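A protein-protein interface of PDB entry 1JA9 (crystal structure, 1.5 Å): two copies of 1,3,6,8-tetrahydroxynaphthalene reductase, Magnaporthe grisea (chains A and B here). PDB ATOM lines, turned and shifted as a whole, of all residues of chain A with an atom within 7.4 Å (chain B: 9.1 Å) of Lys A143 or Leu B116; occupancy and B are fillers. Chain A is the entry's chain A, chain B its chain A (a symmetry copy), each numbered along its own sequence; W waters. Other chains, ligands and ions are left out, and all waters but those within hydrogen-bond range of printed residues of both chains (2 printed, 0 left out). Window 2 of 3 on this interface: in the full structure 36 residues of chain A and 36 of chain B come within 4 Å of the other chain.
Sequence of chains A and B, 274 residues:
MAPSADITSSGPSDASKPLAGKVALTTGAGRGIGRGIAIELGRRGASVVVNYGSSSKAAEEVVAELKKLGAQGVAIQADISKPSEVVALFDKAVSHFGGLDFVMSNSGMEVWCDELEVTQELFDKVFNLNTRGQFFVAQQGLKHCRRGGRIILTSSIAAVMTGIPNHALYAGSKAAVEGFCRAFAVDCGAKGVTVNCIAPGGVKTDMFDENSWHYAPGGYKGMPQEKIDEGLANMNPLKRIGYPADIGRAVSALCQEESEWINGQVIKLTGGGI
Of the 11 printed residues of chain B, 7 touch a printed residue of chain A. Printed residues of chain B that touch a printed residue of chain A: Glu B115, Leu B116, Val B118, Thr B119, Gln B120, Asn B166 and Ala B168. Hydrophobic or aromatic side chains of chain B within 4 Å of the printed part of chain A: Leu B116, Val B118 and Ala B168. Hydrophobic or aromatic side chains of chain A within 4 Å of the printed part of chain B: Phe A135, Phe A136, Leu A142 and Phe A184. Among the printed residues, 16 pairs touch across the chains. Among the printed residues, no Asp or Glu carboxylate lies within 4 Å of a Lys or Arg side-chain nitrogen of the other chain.
The backbone carbonyl oxygen (O) of Glu B115 lies close to the side-chain amide oxygen (OE1) of Gln A139 (2.9 Å). The side-chain amide oxygen (OE1) of Gln A139 sits close to the backbone carbonyl oxygen (O) of Leu B116, 3.4 Å away. The backbone carbonyl oxygen of Val B118 lies close to the side-chain amide oxygen of Gln A139, at 3.0 Å. OD1 of Asp A187 lies close to OE1 of Glu B115, at 2.7 Å. OD2 of Asp A187 is in hydrogen-bond range of N of Asn B166 (2.8 Å).
Water W2 lies within hydrogen-bond range of N of Glu B115, ND2 of Asn B166 and OD2 of Asp A187. Water W1 lies within hydrogen-bond range of the side-chain carboxylate of Asp A187 (2.9 Å) and the backbone NH of Asn B166 (3.1 Å).
Lys A143 touches one residue of chain B. Leu B116 touches just these residues of chain A: Gln A139 (3.4 Å), Leu A142 (3.9 Å) and Lys A143 (3.6 Å). No residue of chain B comes within 4 Å of Gly A141. Of chain B, only Glu B115 (3.95 Å) and Leu B116 (3.9 Å) come within 4 Å of Leu A142. No residue of chain B comes within 4 Å of His A144. Of the printed residues of chain B, Asp A187 touches Glu B115 (2.7 Å) and Asn B166 (2.8 Å). Printed residues of chain A within 4 Å of Asn B166: Asp A187 (2.8 Å). The nearest printed residue of chain A that does not touch Glu B115 is Phe A136 (6.1 Å).
NE2 of Gln A139 sits close to NE2 of Gln A140 (3.0 Å). The backbone carbonyl oxygen of Phe A184 lies within hydrogen-bond range of the side-chain sulfur of Cys A188 (3.3 Å). N of Cys B113 lies within hydrogen-bond range of O of Asn B166 (2.9 Å). The side-chain carboxylate (OD1) of Asp B114 lies within hydrogen-bond range of the backbone NH (N) of Leu B116, 3.0 Å away. The backbone NH of Ala B168 is in hydrogen-bond range of the side-chain carboxylate of Glu B115 (3.1 Å). N of Leu B122 lies within hydrogen-bond range of OG1 of Thr B119 (3.1 Å).
No position is printed for both chains. Of the 16 pairs that touch across the chains among the printed residues, none has its exchanged pair printed and touching as well.
Phe A135 touches Glu B115 (CE1 to OE2, 3.5 Å). Phe A135 touches Val B118 (CE2 to CG1, 3.5 Å). Val B118 touches Phe A136. Phe A136 touches Thr B119 (CZ to C, 3.8 Å). CZ of Phe A136 touches N of Gln B120, at 3.8 Å. Glu B115 touches Leu A142. Leu A142 touches Leu B116. Lys A143 touches Leu B116. CE2 of Phe A184 touches CB of Glu B115, 3.6 Å away. Ala B168 touches Phe A184 (CB to CE1, 3.7 Å).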
ATOM      1  N   VAL A  87     -27.848  23.719  14.734  1.00  0.00           N
ATOM      2  CA  VAL A  87     -27.698  22.497  13.970  1.00  0.00           C
ATOM      3  C   VAL A  87     -27.201  22.822  12.547  1.00  0.00           C
ATOM      4  O   VAL A  87     -26.280  22.163  12.039  1.00  0.00           O
ATOM      5  CB  VAL A  87     -29.000  21.710  13.920  1.00  0.00           C
ATOM      6  CG1 VAL A  87     -28.855  20.525  12.984  1.00  0.00           C
ATOM      7  CG2 VAL A  87     -29.376  21.239  15.333  1.00  0.00           C
ATOM      8  N   PHE A  90     -23.435  23.728  12.448  1.00  0.00           N
ATOM      9  CA  PHE A  90     -22.569  22.560  12.456  1.00  0.00           C
ATOM     10  C   PHE A  90     -22.553  21.820  11.126  1.00  0.00           C
ATOM     11  O   PHE A  90     -21.500  21.385  10.674  1.00  0.00           O
ATOM     12  CB  PHE A  90     -22.911  21.618  13.598  1.00  0.00           C
ATOM     13  CG  PHE A  90     -22.302  22.038  14.918  1.00  0.00           C
ATOM     14  CD1 PHE A  90     -22.767  23.174  15.598  1.00  0.00           C
ATOM     15  CD2 PHE A  90     -21.238  21.317  15.463  1.00  0.00           C
ATOM     16  CE1 PHE A  90     -22.174  23.588  16.809  1.00  0.00           C
ATOM     17  CE2 PHE A  90     -20.640  21.735  16.677  1.00  0.00           C
ATOM     18  CZ  PHE A  90     -21.124  22.877  17.339  1.00  0.00           C
ATOM     19  N   ASP A  91     -23.713  21.688  10.500  1.00  0.00           N
ATOM     20  CA  ASP A  91     -23.794  21.023   9.198  1.00  0.00           C
ATOM     21  C   ASP A  91     -22.895  21.739   8.183  1.00  0.00           C
ATOM     22  O   ASP A  91     -22.158  21.099   7.431  1.00  0.00           O
ATOM     23  CB  ASP A  91     -25.230  21.032   8.706  1.00  0.00           C
ATOM     24  CG  ASP A  91     -26.138  20.125   9.516  1.00  0.00           C
ATOM     25  OD1 ASP A  91     -25.677  19.113  10.066  1.00  0.00           O
ATOM     26  OD2 ASP A  91     -27.348  20.403   9.549  1.00  0.00           O
ATOM     27  N   PHE A 135     -26.320  24.401  25.404  1.00  0.00           N
ATOM     28  CA  PHE A 135     -26.731  23.002  25.435  1.00  0.00           C
ATOM     29  C   PHE A 135     -26.688  22.434  24.007  1.00  0.00           C
ATOM     30  O   PHE A 135     -26.116  21.370  23.776  1.00  0.00           O
ATOM     31  CB  PHE A 135     -28.153  22.822  25.981  1.00  0.00           C
ATOM     32  CG  PHE A 135     -28.631  21.395  25.904  1.00  0.00           C
ATOM     33  CD1 PHE A 135     -28.310  20.476  26.913  1.00  0.00           C
ATOM     34  CD2 PHE A 135     -29.254  20.925  24.736  1.00  0.00           C
ATOM     35  CE1 PHE A 135     -28.581  19.123  26.753  1.00  0.00           C
ATOM     36  CE2 PHE A 135     -29.527  19.568  24.567  1.00  0.00           C
ATOM     37  CZ  PHE A 135     -29.187  18.668  25.567  1.00  0.00           C
ATOM     38  N   PHE A 136     -27.275  23.152  23.056  1.00  0.00           N
ATOM     39  CA  PHE A 136     -27.295  22.670  21.675  1.00  0.00           C
ATOM     40  C   PHE A 136     -25.942  22.674  20.995  1.00  0.00           C
ATOM     41  O   PHE A 136     -25.654  21.790  20.184  1.00  0.00           O
ATOM     42  CB  PHE A 136     -28.415  23.358  20.876  1.00  0.00           C
ATOM     43  CG  PHE A 136     -29.779  22.830  21.241  1.00  0.00           C
ATOM     44  CD1 PHE A 136     -30.575  23.490  22.181  1.00  0.00           C
ATOM     45  CD2 PHE A 136     -30.209  21.598  20.745  1.00  0.00           C
ATOM     46  CE1 PHE A 136     -31.769  22.907  22.622  1.00  0.00           C
ATOM     47  CE2 PHE A 136     -31.393  21.020  21.179  1.00  0.00           C
ATOM     48  CZ  PHE A 136     -32.180  21.679  22.129  1.00  0.00           C
ATOM     49  N   VAL A 137     -25.100  23.640  21.330  1.00  0.00           N
ATOM     50  CA  VAL A 137     -23.744  23.641  20.790  1.00  0.00           C
ATOM     51  C   VAL A 137     -23.050  22.354  21.342  1.00  0.00           C
ATOM     52  O   VAL A 137     -22.376  21.617  20.600  1.00  0.00           O
ATOM     53  CB  VAL A 137     -23.003  24.929  21.210  1.00  0.00           C
ATOM     54  CG1 VAL A 137     -21.491  24.850  20.921  1.00  0.00           C
ATOM     55  CG2 VAL A 137     -23.604  26.117  20.457  1.00  0.00           C
ATOM     56  N   ALA A 138     -23.263  22.042  22.623  1.00  0.00           N
ATOM     57  CA  ALA A 138     -22.649  20.860  23.212  1.00  0.00           C
ATOM     58  C   ALA A 138     -23.208  19.575  22.563  1.00  0.00           C
ATOM     59  O   ALA A 138     -22.463  18.622  22.303  1.00  0.00           O
ATOM     60  CB  ALA A 138     -22.834  20.857  24.751  1.00  0.00           C
ATOM     61  N   GLN A 139     -24.523  19.550  22.309  1.00  0.00           N
ATOM     62  CA  GLN A 139     -25.151  18.393  21.668  1.00  0.00           C
ATOM     63  C   GLN A 139     -24.494  18.198  20.304  1.00  0.00           C
ATOM     64  O   GLN A 139     -24.157  17.068  19.946  1.00  0.00           O
ATOM     65  CB  GLN A 139     -26.646  18.634  21.451  1.00  0.00           C
ATOM     66  CG  GLN A 139     -27.373  17.532  20.651  1.00  0.00           C
ATOM     67  CD  GLN A 139     -28.758  17.985  20.227  1.00  0.00           C
ATOM     68  OE1 GLN A 139     -29.786  17.567  20.805  1.00  0.00           O
ATOM     69  NE2 GLN A 139     -28.800  18.881  19.261  1.00  0.00           N
ATOM     70  N   GLN A 140     -24.319  19.296  19.564  1.00  0.00           N
ATOM     71  CA  GLN A 140     -23.715  19.216  18.236  1.00  0.00           C
ATOM     72  C   GLN A 140     -22.254  18.777  18.317  1.00  0.00           C
ATOM     73  O   GLN A 140     -21.772  18.044  17.445  1.00  0.00           O
ATOM     74  CB  GLN A 140     -23.927  20.515  17.459  1.00  0.00           C
ATOM     75  CG  GLN A 140     -25.444  20.757  17.153  1.00  0.00           C
ATOM     76  CD  GLN A 140     -26.053  19.638  16.296  1.00  0.00           C
ATOM     77  OE1 GLN A 140     -25.601  19.410  15.174  1.00  0.00           O
ATOM     78  NE2 GLN A 140     -27.026  18.910  16.837  1.00  0.00           N
ATOM     79  N   GLY A 141     -21.569  19.160  19.396  1.00  0.00           N
ATOM     80  CA  GLY A 141     -20.197  18.714  19.584  1.00  0.00           C
ATOM     81  C   GLY A 141     -20.200  17.206  19.811  1.00  0.00           C
ATOM     82  O   GLY A 141     -19.339  16.491  19.306  1.00  0.00           O
ATOM     83  N   LEU A 142     -21.124  16.703  20.620  1.00  0.00           N
ATOM     84  CA  LEU A 142     -21.202  15.252  20.865  1.00  0.00           C
ATOM     85  C   LEU A 142     -21.489  14.544  19.545  1.00  0.00           C
ATOM     86  O   LEU A 142     -20.973  13.464  19.286  1.00  0.00           O
ATOM     87  CB  LEU A 142     -22.324  14.918  21.855  1.00  0.00           C
ATOM     88  CG  LEU A 142     -22.750  13.454  22.044  1.00  0.00           C
ATOM     89  CD1 LEU A 142     -21.591  12.542  22.448  1.00  0.00           C
ATOM     90  CD2 LEU A 142     -23.902  13.412  23.086  1.00  0.00           C
ATOM     91  N   LYS A 143     -22.340  15.161  18.731  1.00  0.00           N
ATOM     92  CA  LYS A 143     -22.724  14.574  17.456  1.00  0.00           C
ATOM     93  C   LYS A 143     -21.591  14.525  16.445  1.00  0.00           C
ATOM     94  O   LYS A 143     -21.454  13.521  15.754  1.00  0.00           O
ATOM     95  CB  LYS A 143     -23.905  15.353  16.859  1.00  0.00           C
ATOM     96  CG  LYS A 143     -24.452  14.767  15.563  1.00  0.00           C
ATOM     97  CD  LYS A 143     -25.563  15.671  15.020  1.00  0.00           C
ATOM     98  CE  LYS A 143     -26.096  15.160  13.705  1.00  0.00           C
ATOM     99  NZ  LYS A 143     -27.144  16.093  13.218  1.00  0.00           N
ATOM    100  N   HIS A 144     -20.745  15.557  16.422  1.00  0.00           N
ATOM    101  CA  HIS A 144     -19.681  15.668  15.414  1.00  0.00           C
ATOM    102  C   HIS A 144     -18.204  15.580  15.814  1.00  0.00           C
ATOM    103  O   HIS A 144     -17.375  15.259  14.969  1.00  0.00           O
ATOM    104  CB  HIS A 144     -19.858  16.995  14.621  1.00  0.00           C
ATOM    105  CG  HIS A 144     -21.137  17.086  13.841  1.00  0.00           C
ATOM    106  ND1 HIS A 144     -21.366  16.346  12.701  1.00  0.00           N
ATOM    107  CD2 HIS A 144     -22.258  17.826  14.039  1.00  0.00           C
ATOM    108  CE1 HIS A 144     -22.573  16.618  12.233  1.00  0.00           C
ATOM    109  NE2 HIS A 144     -23.135  17.515  13.023  1.00  0.00           N
ATOM    110  N   CYS A 145     -17.851  15.923  17.052  1.00  0.00           N
ATOM    111  CA  CYS A 145     -16.444  15.912  17.448  1.00  0.00           C
ATOM    112  C   CYS A 145     -15.756  14.574  17.247  1.00  0.00           C
ATOM    113  O   CYS A 145     -16.253  13.533  17.691  1.00  0.00           O
ATOM    114  CB  CYS A 145     -16.266  16.349  18.910  1.00  0.00           C
ATOM    115  SG  CYS A 145     -16.542  18.103  19.144  1.00  0.00           S
ATOM    116  N   ARG A 146     -14.587  14.628  16.620  1.00  0.00           N
ATOM    117  CA  ARG A 146     -13.808  13.424  16.385  1.00  0.00           C
ATOM    118  C   ARG A 146     -13.092  13.025  17.653  1.00  0.00           C
ATOM    119  O   ARG A 146     -12.934  13.852  18.569  1.00  0.00           O
ATOM    120  CB  ARG A 146     -12.797  13.674  15.272  1.00  0.00           C
ATOM    121  CG  ARG A 146     -13.494  13.941  13.950  1.00  0.00           C
ATOM    122  CD  ARG A 146     -12.508  14.050  12.816  1.00  0.00           C
ATOM    123  NE  ARG A 146     -11.759  15.301  12.797  1.00  0.00           N
ATOM    124  CZ  ARG A 146     -11.488  15.973  11.677  1.00  0.00           C
ATOM    125  NH1 ARG A 146     -11.919  15.515  10.500  1.00  0.00           N
ATOM    126  NH2 ARG A 146     -10.721  17.059  11.717  1.00  0.00           N
ATOM    127  N   ILE A 151     -14.801  19.852  23.915  1.00  0.00           N
ATOM    128  CA  ILE A 151     -15.959  20.750  23.947  1.00  0.00           C
ATOM    129  C   ILE A 151     -15.698  21.597  25.188  1.00  0.00           C
ATOM    130  O   ILE A 151     -15.384  21.060  26.269  1.00  0.00           O
ATOM    131  CB  ILE A 151     -17.292  20.000  24.126  1.00  0.00           C
ATOM    132  CG1 ILE A 151     -17.570  19.095  22.911  1.00  0.00           C
ATOM    133  CG2 ILE A 151     -18.440  21.032  24.349  1.00  0.00           C
ATOM    134  CD1 ILE A 151     -18.770  18.172  23.094  1.00  0.00           C
ATOM    135  N   PHE A 184     -22.306  16.345  30.198  1.00  0.00           N
ATOM    136  CA  PHE A 184     -21.759  16.069  28.885  1.00  0.00           C
ATOM    137  C   PHE A 184     -20.427  15.337  28.939  1.00  0.00           C
ATOM    138  O   PHE A 184     -20.126  14.579  28.041  1.00  0.00           O
ATOM    139  CB  PHE A 184     -21.652  17.342  28.045  1.00  0.00           C
ATOM    140  CG  PHE A 184     -22.891  17.619  27.242  1.00  0.00           C
ATOM    141  CD1 PHE A 184     -23.908  18.408  27.766  1.00  0.00           C
ATOM    142  CD2 PHE A 184     -23.054  17.082  25.947  1.00  0.00           C
ATOM    143  CE1 PHE A 184     -25.075  18.670  27.021  1.00  0.00           C
ATOM    144  CE2 PHE A 184     -24.222  17.345  25.197  1.00  0.00           C
ATOM    145  CZ  PHE A 184     -25.222  18.138  25.736  1.00  0.00           C
ATOM    146  N   ASP A 187     -21.376  11.873  28.982  1.00  0.00           N
ATOM    147  CA  ASP A 187     -21.998  11.539  27.698  1.00  0.00           C
ATOM    148  C   ASP A 187     -21.077  11.484  26.476  1.00  0.00           C
ATOM    149  O   ASP A 187     -21.383  10.816  25.494  1.00  0.00           O
ATOM    150  CB  ASP A 187     -23.195  12.469  27.447  1.00  0.00           C
ATOM    151  CG  ASP A 187     -24.267  12.307  28.523  1.00  0.00           C
ATOM    152  OD1 ASP A 187     -24.820  13.327  28.974  1.00  0.00           O
ATOM    153  OD2 ASP A 187     -24.522  11.155  28.946  1.00  0.00           O
ATOM    154  N   CYS A 188     -19.957  12.187  26.552  1.00  0.00           N
ATOM    155  CA  CYS A 188     -18.999  12.241  25.457  1.00  0.00           C
ATOM    156  C   CYS A 188     -17.841  11.277  25.621  1.00  0.00           C
ATOM    157  O   CYS A 188     -17.014  11.162  24.729  1.00  0.00           O
ATOM    158  CB  CYS A 188     -18.428  13.661  25.344  1.00  0.00           C
ATOM    159  SG  CYS A 188     -19.639  14.883  24.840  1.00  0.00           S
ATOM    160  N   LYS A 191     -16.998   8.550  22.997  1.00  0.00           N
ATOM    161  CA  LYS A 191     -16.465   9.132  21.773  1.00  0.00           C
ATOM    162  C   LYS A 191     -15.053   9.676  21.950  1.00  0.00           C
ATOM    163  O   LYS A 191     -14.450  10.145  21.003  1.00  0.00           O
ATOM    164  CB  LYS A 191     -17.392  10.240  21.284  1.00  0.00           C
ATOM    165  CG  LYS A 191     -18.704   9.741  20.692  1.00  0.00           C
ATOM    166  CD  LYS A 191     -18.480   9.183  19.275  1.00  0.00           C
ATOM    167  CE  LYS A 191     -19.751   8.570  18.730  1.00  0.00           C
ATOM    168  NZ  LYS A 191     -19.747   8.558  17.242  1.00  0.00           N
ATOM    169  N   CYS B 113     -32.447  11.639  29.161  1.00  0.00           N
ATOM    170  CA  CYS B 113     -32.497  11.626  27.704  1.00  0.00           C
ATOM    171  C   CYS B 113     -31.098  11.663  27.088  1.00  0.00           C
ATOM    172  O   CYS B 113     -30.199  12.379  27.564  1.00  0.00           O
ATOM    173  CB  CYS B 113     -33.305  12.829  27.183  1.00  0.00           C
ATOM    174  SG  CYS B 113     -33.699  12.762  25.393  1.00  0.00           S
ATOM    175  N   ASP B 114     -30.931  10.852  26.042  1.00  0.00           N
ATOM    176  CA  ASP B 114     -29.695  10.819  25.268  1.00  0.00           C
ATOM    177  C   ASP B 114     -29.577  12.266  24.814  1.00  0.00           C
ATOM    178  O   ASP B 114     -30.509  12.801  24.230  1.00  0.00           O
ATOM    179  CB  ASP B 114     -29.922   9.915  24.047  1.00  0.00           C
ATOM    180  CG  ASP B 114     -28.681   9.728  23.201  1.00  0.00           C
ATOM    181  OD1 ASP B 114     -27.891  10.665  22.981  1.00  0.00           O
ATOM    182  OD2 ASP B 114     -28.531   8.597  22.708  1.00  0.00           O
ATOM    183  N   GLU B 115     -28.450  12.923  25.069  1.00  0.00           N
ATOM    184  CA  GLU B 115     -28.336  14.341  24.668  1.00  0.00           C
ATOM    185  C   GLU B 115     -28.630  14.589  23.187  1.00  0.00           C
ATOM    186  O   GLU B 115     -29.203  15.624  22.838  1.00  0.00           O
ATOM    187  CB  GLU B 115     -26.967  14.958  25.044  1.00  0.00           C
ATOM    188  CG  GLU B 115     -26.464  14.651  26.463  1.00  0.00           C
ATOM    189  CD  GLU B 115     -27.444  15.011  27.611  1.00  0.00           C
ATOM    190  OE1 GLU B 115     -27.208  14.555  28.762  1.00  0.00           O
ATOM    191  OE2 GLU B 115     -28.436  15.727  27.393  1.00  0.00           O
ATOM    192  N   LEU B 116     -28.290  13.617  22.331  1.00  0.00           N
ATOM    193  CA  LEU B 116     -28.515  13.754  20.882  1.00  0.00           C
ATOM    194  C   LEU B 116     -29.981  13.825  20.540  1.00  0.00           C
ATOM    195  O   LEU B 116     -30.345  14.448  19.538  1.00  0.00           O
ATOM    196  CB  LEU B 116     -27.888  12.582  20.121  1.00  0.00           C
ATOM    197  CG  LEU B 116     -26.348  12.530  20.128  1.00  0.00           C
ATOM    198  CD1 LEU B 116     -25.817  11.291  19.387  1.00  0.00           C
ATOM    199  CD2 LEU B 116     -25.788  13.790  19.497  1.00  0.00           C
ATOM    200  N   GLU B 117     -30.804  13.250  21.416  1.00  0.00           N
ATOM    201  CA  GLU B 117     -32.254  13.180  21.214  1.00  0.00           C
ATOM    202  C   GLU B 117     -33.063  14.313  21.838  1.00  0.00           C
ATOM    203  O   GLU B 117     -34.264  14.437  21.610  1.00  0.00           O
ATOM    204  CB  GLU B 117     -32.773  11.829  21.683  1.00  0.00           C
ATOM    205  CG  GLU B 117     -32.209  10.679  20.858  1.00  0.00           C
ATOM    206  CD  GLU B 117     -32.538   9.310  21.418  1.00  0.00           C
ATOM    207  OE1 GLU B 117     -33.291   9.202  22.422  1.00  0.00           O
ATOM    208  OE2 GLU B 117     -32.026   8.318  20.849  1.00  0.00           O
ATOM    209  N   VAL B 118     -32.398  15.152  22.620  1.00  0.00           N
ATOM    210  CA  VAL B 118     -33.086  16.275  23.241  1.00  0.00           C
ATOM    211  C   VAL B 118     -33.539  17.278  22.173  1.00  0.00           C
ATOM    212  O   VAL B 118     -32.764  17.714  21.322  1.00  0.00           O
ATOM    213  CB  VAL B 118     -32.174  17.003  24.314  1.00  0.00           C
ATOM    214  CG1 VAL B 118     -32.827  18.329  24.782  1.00  0.00           C
ATOM    215  CG2 VAL B 118     -31.896  16.077  25.496  1.00  0.00           C
ATOM    216  N   THR B 119     -34.815  17.640  22.250  1.00  0.00           N
ATOM    217  CA  THR B 119     -35.410  18.602  21.355  1.00  0.00           C
ATOM    218  C   THR B 119     -35.585  19.926  22.113  1.00  0.00           C
ATOM    219  O   THR B 119     -35.533  19.967  23.357  1.00  0.00           O
ATOM    220  CB  THR B 119     -36.800  18.133  20.965  1.00  0.00           C
ATOM    221  OG1 THR B 119     -37.588  17.961  22.156  1.00  0.00           O
ATOM    222  CG2 THR B 119     -36.727  16.820  20.231  1.00  0.00           C
ATOM    223  N   GLN B 120     -35.842  21.002  21.381  1.00  0.00           N
ATOM    224  CA  GLN B 120     -36.071  22.285  22.026  1.00  0.00           C
ATOM    225  C   GLN B 120     -37.295  22.149  22.939  1.00  0.00           C
ATOM    226  O   GLN B 120     -37.356  22.740  24.017  1.00  0.00           O
ATOM    227  CB  GLN B 120     -36.369  23.375  21.004  1.00  0.00           C
ATOM    228  CG  GLN B 120     -36.587  24.713  21.657  1.00  0.00           C
ATOM    229  CD  GLN B 120     -37.077  25.761  20.711  1.00  0.00           C
ATOM    230  OE1 GLN B 120     -36.543  25.941  19.640  1.00  0.00           O
ATOM    231  NE2 GLN B 120     -38.069  26.496  21.129  1.00  0.00           N
ATOM    232  N   LEU B 122     -38.417  19.533  24.652  1.00  0.00           N
ATOM    233  CA  LEU B 122     -38.081  18.875  25.918  1.00  0.00           C
ATOM    234  C   LEU B 122     -37.270  19.853  26.797  1.00  0.00           C
ATOM    235  O   LEU B 122     -37.539  19.996  27.984  1.00  0.00           O
ATOM    236  CB  LEU B 122     -37.260  17.614  25.664  1.00  0.00           C
ATOM    237  CG  LEU B 122     -36.878  16.832  26.925  1.00  0.00           C
ATOM    238  CD1 LEU B 122     -38.131  16.462  27.761  1.00  0.00           C
ATOM    239  CD2 LEU B 122     -36.076  15.597  26.536  1.00  0.00           C
ATOM    240  N   ASN B 166     -26.853  10.866  30.489  1.00  0.00           N
ATOM    241  CA  ASN B 166     -28.163  11.275  29.944  1.00  0.00           C
ATOM    242  C   ASN B 166     -28.954  12.192  30.894  1.00  0.00           C
ATOM    243  O   ASN B 166     -30.204  12.202  30.883  1.00  0.00           O
ATOM    244  CB  ASN B 166     -28.984  10.006  29.680  1.00  0.00           C
ATOM    245  CG  ASN B 166     -28.197   8.970  28.886  1.00  0.00           C
ATOM    246  OD1 ASN B 166     -27.999   7.833  29.336  1.00  0.00           O
ATOM    247  ND2 ASN B 166     -27.685   9.384  27.746  1.00  0.00           N
ATOM    248  N   ALA B 168     -28.107  15.859  31.393  1.00  0.00           N
ATOM    249  CA  ALA B 168     -27.729  17.258  31.302  1.00  0.00           C
ATOM    250  C   ALA B 168     -28.870  18.239  31.543  1.00  0.00           C
ATOM    251  O   ALA B 168     -28.637  19.307  32.140  1.00  0.00           O
ATOM    252  CB  ALA B 168     -27.031  17.560  29.996  1.00  0.00           C
HETATM  253  O   HOH W   1     -25.368  13.269  31.809  1.00  0.00           O
HETATM  254  O   HOH W   2     -26.332  11.411  26.252  1.00  0.00           O
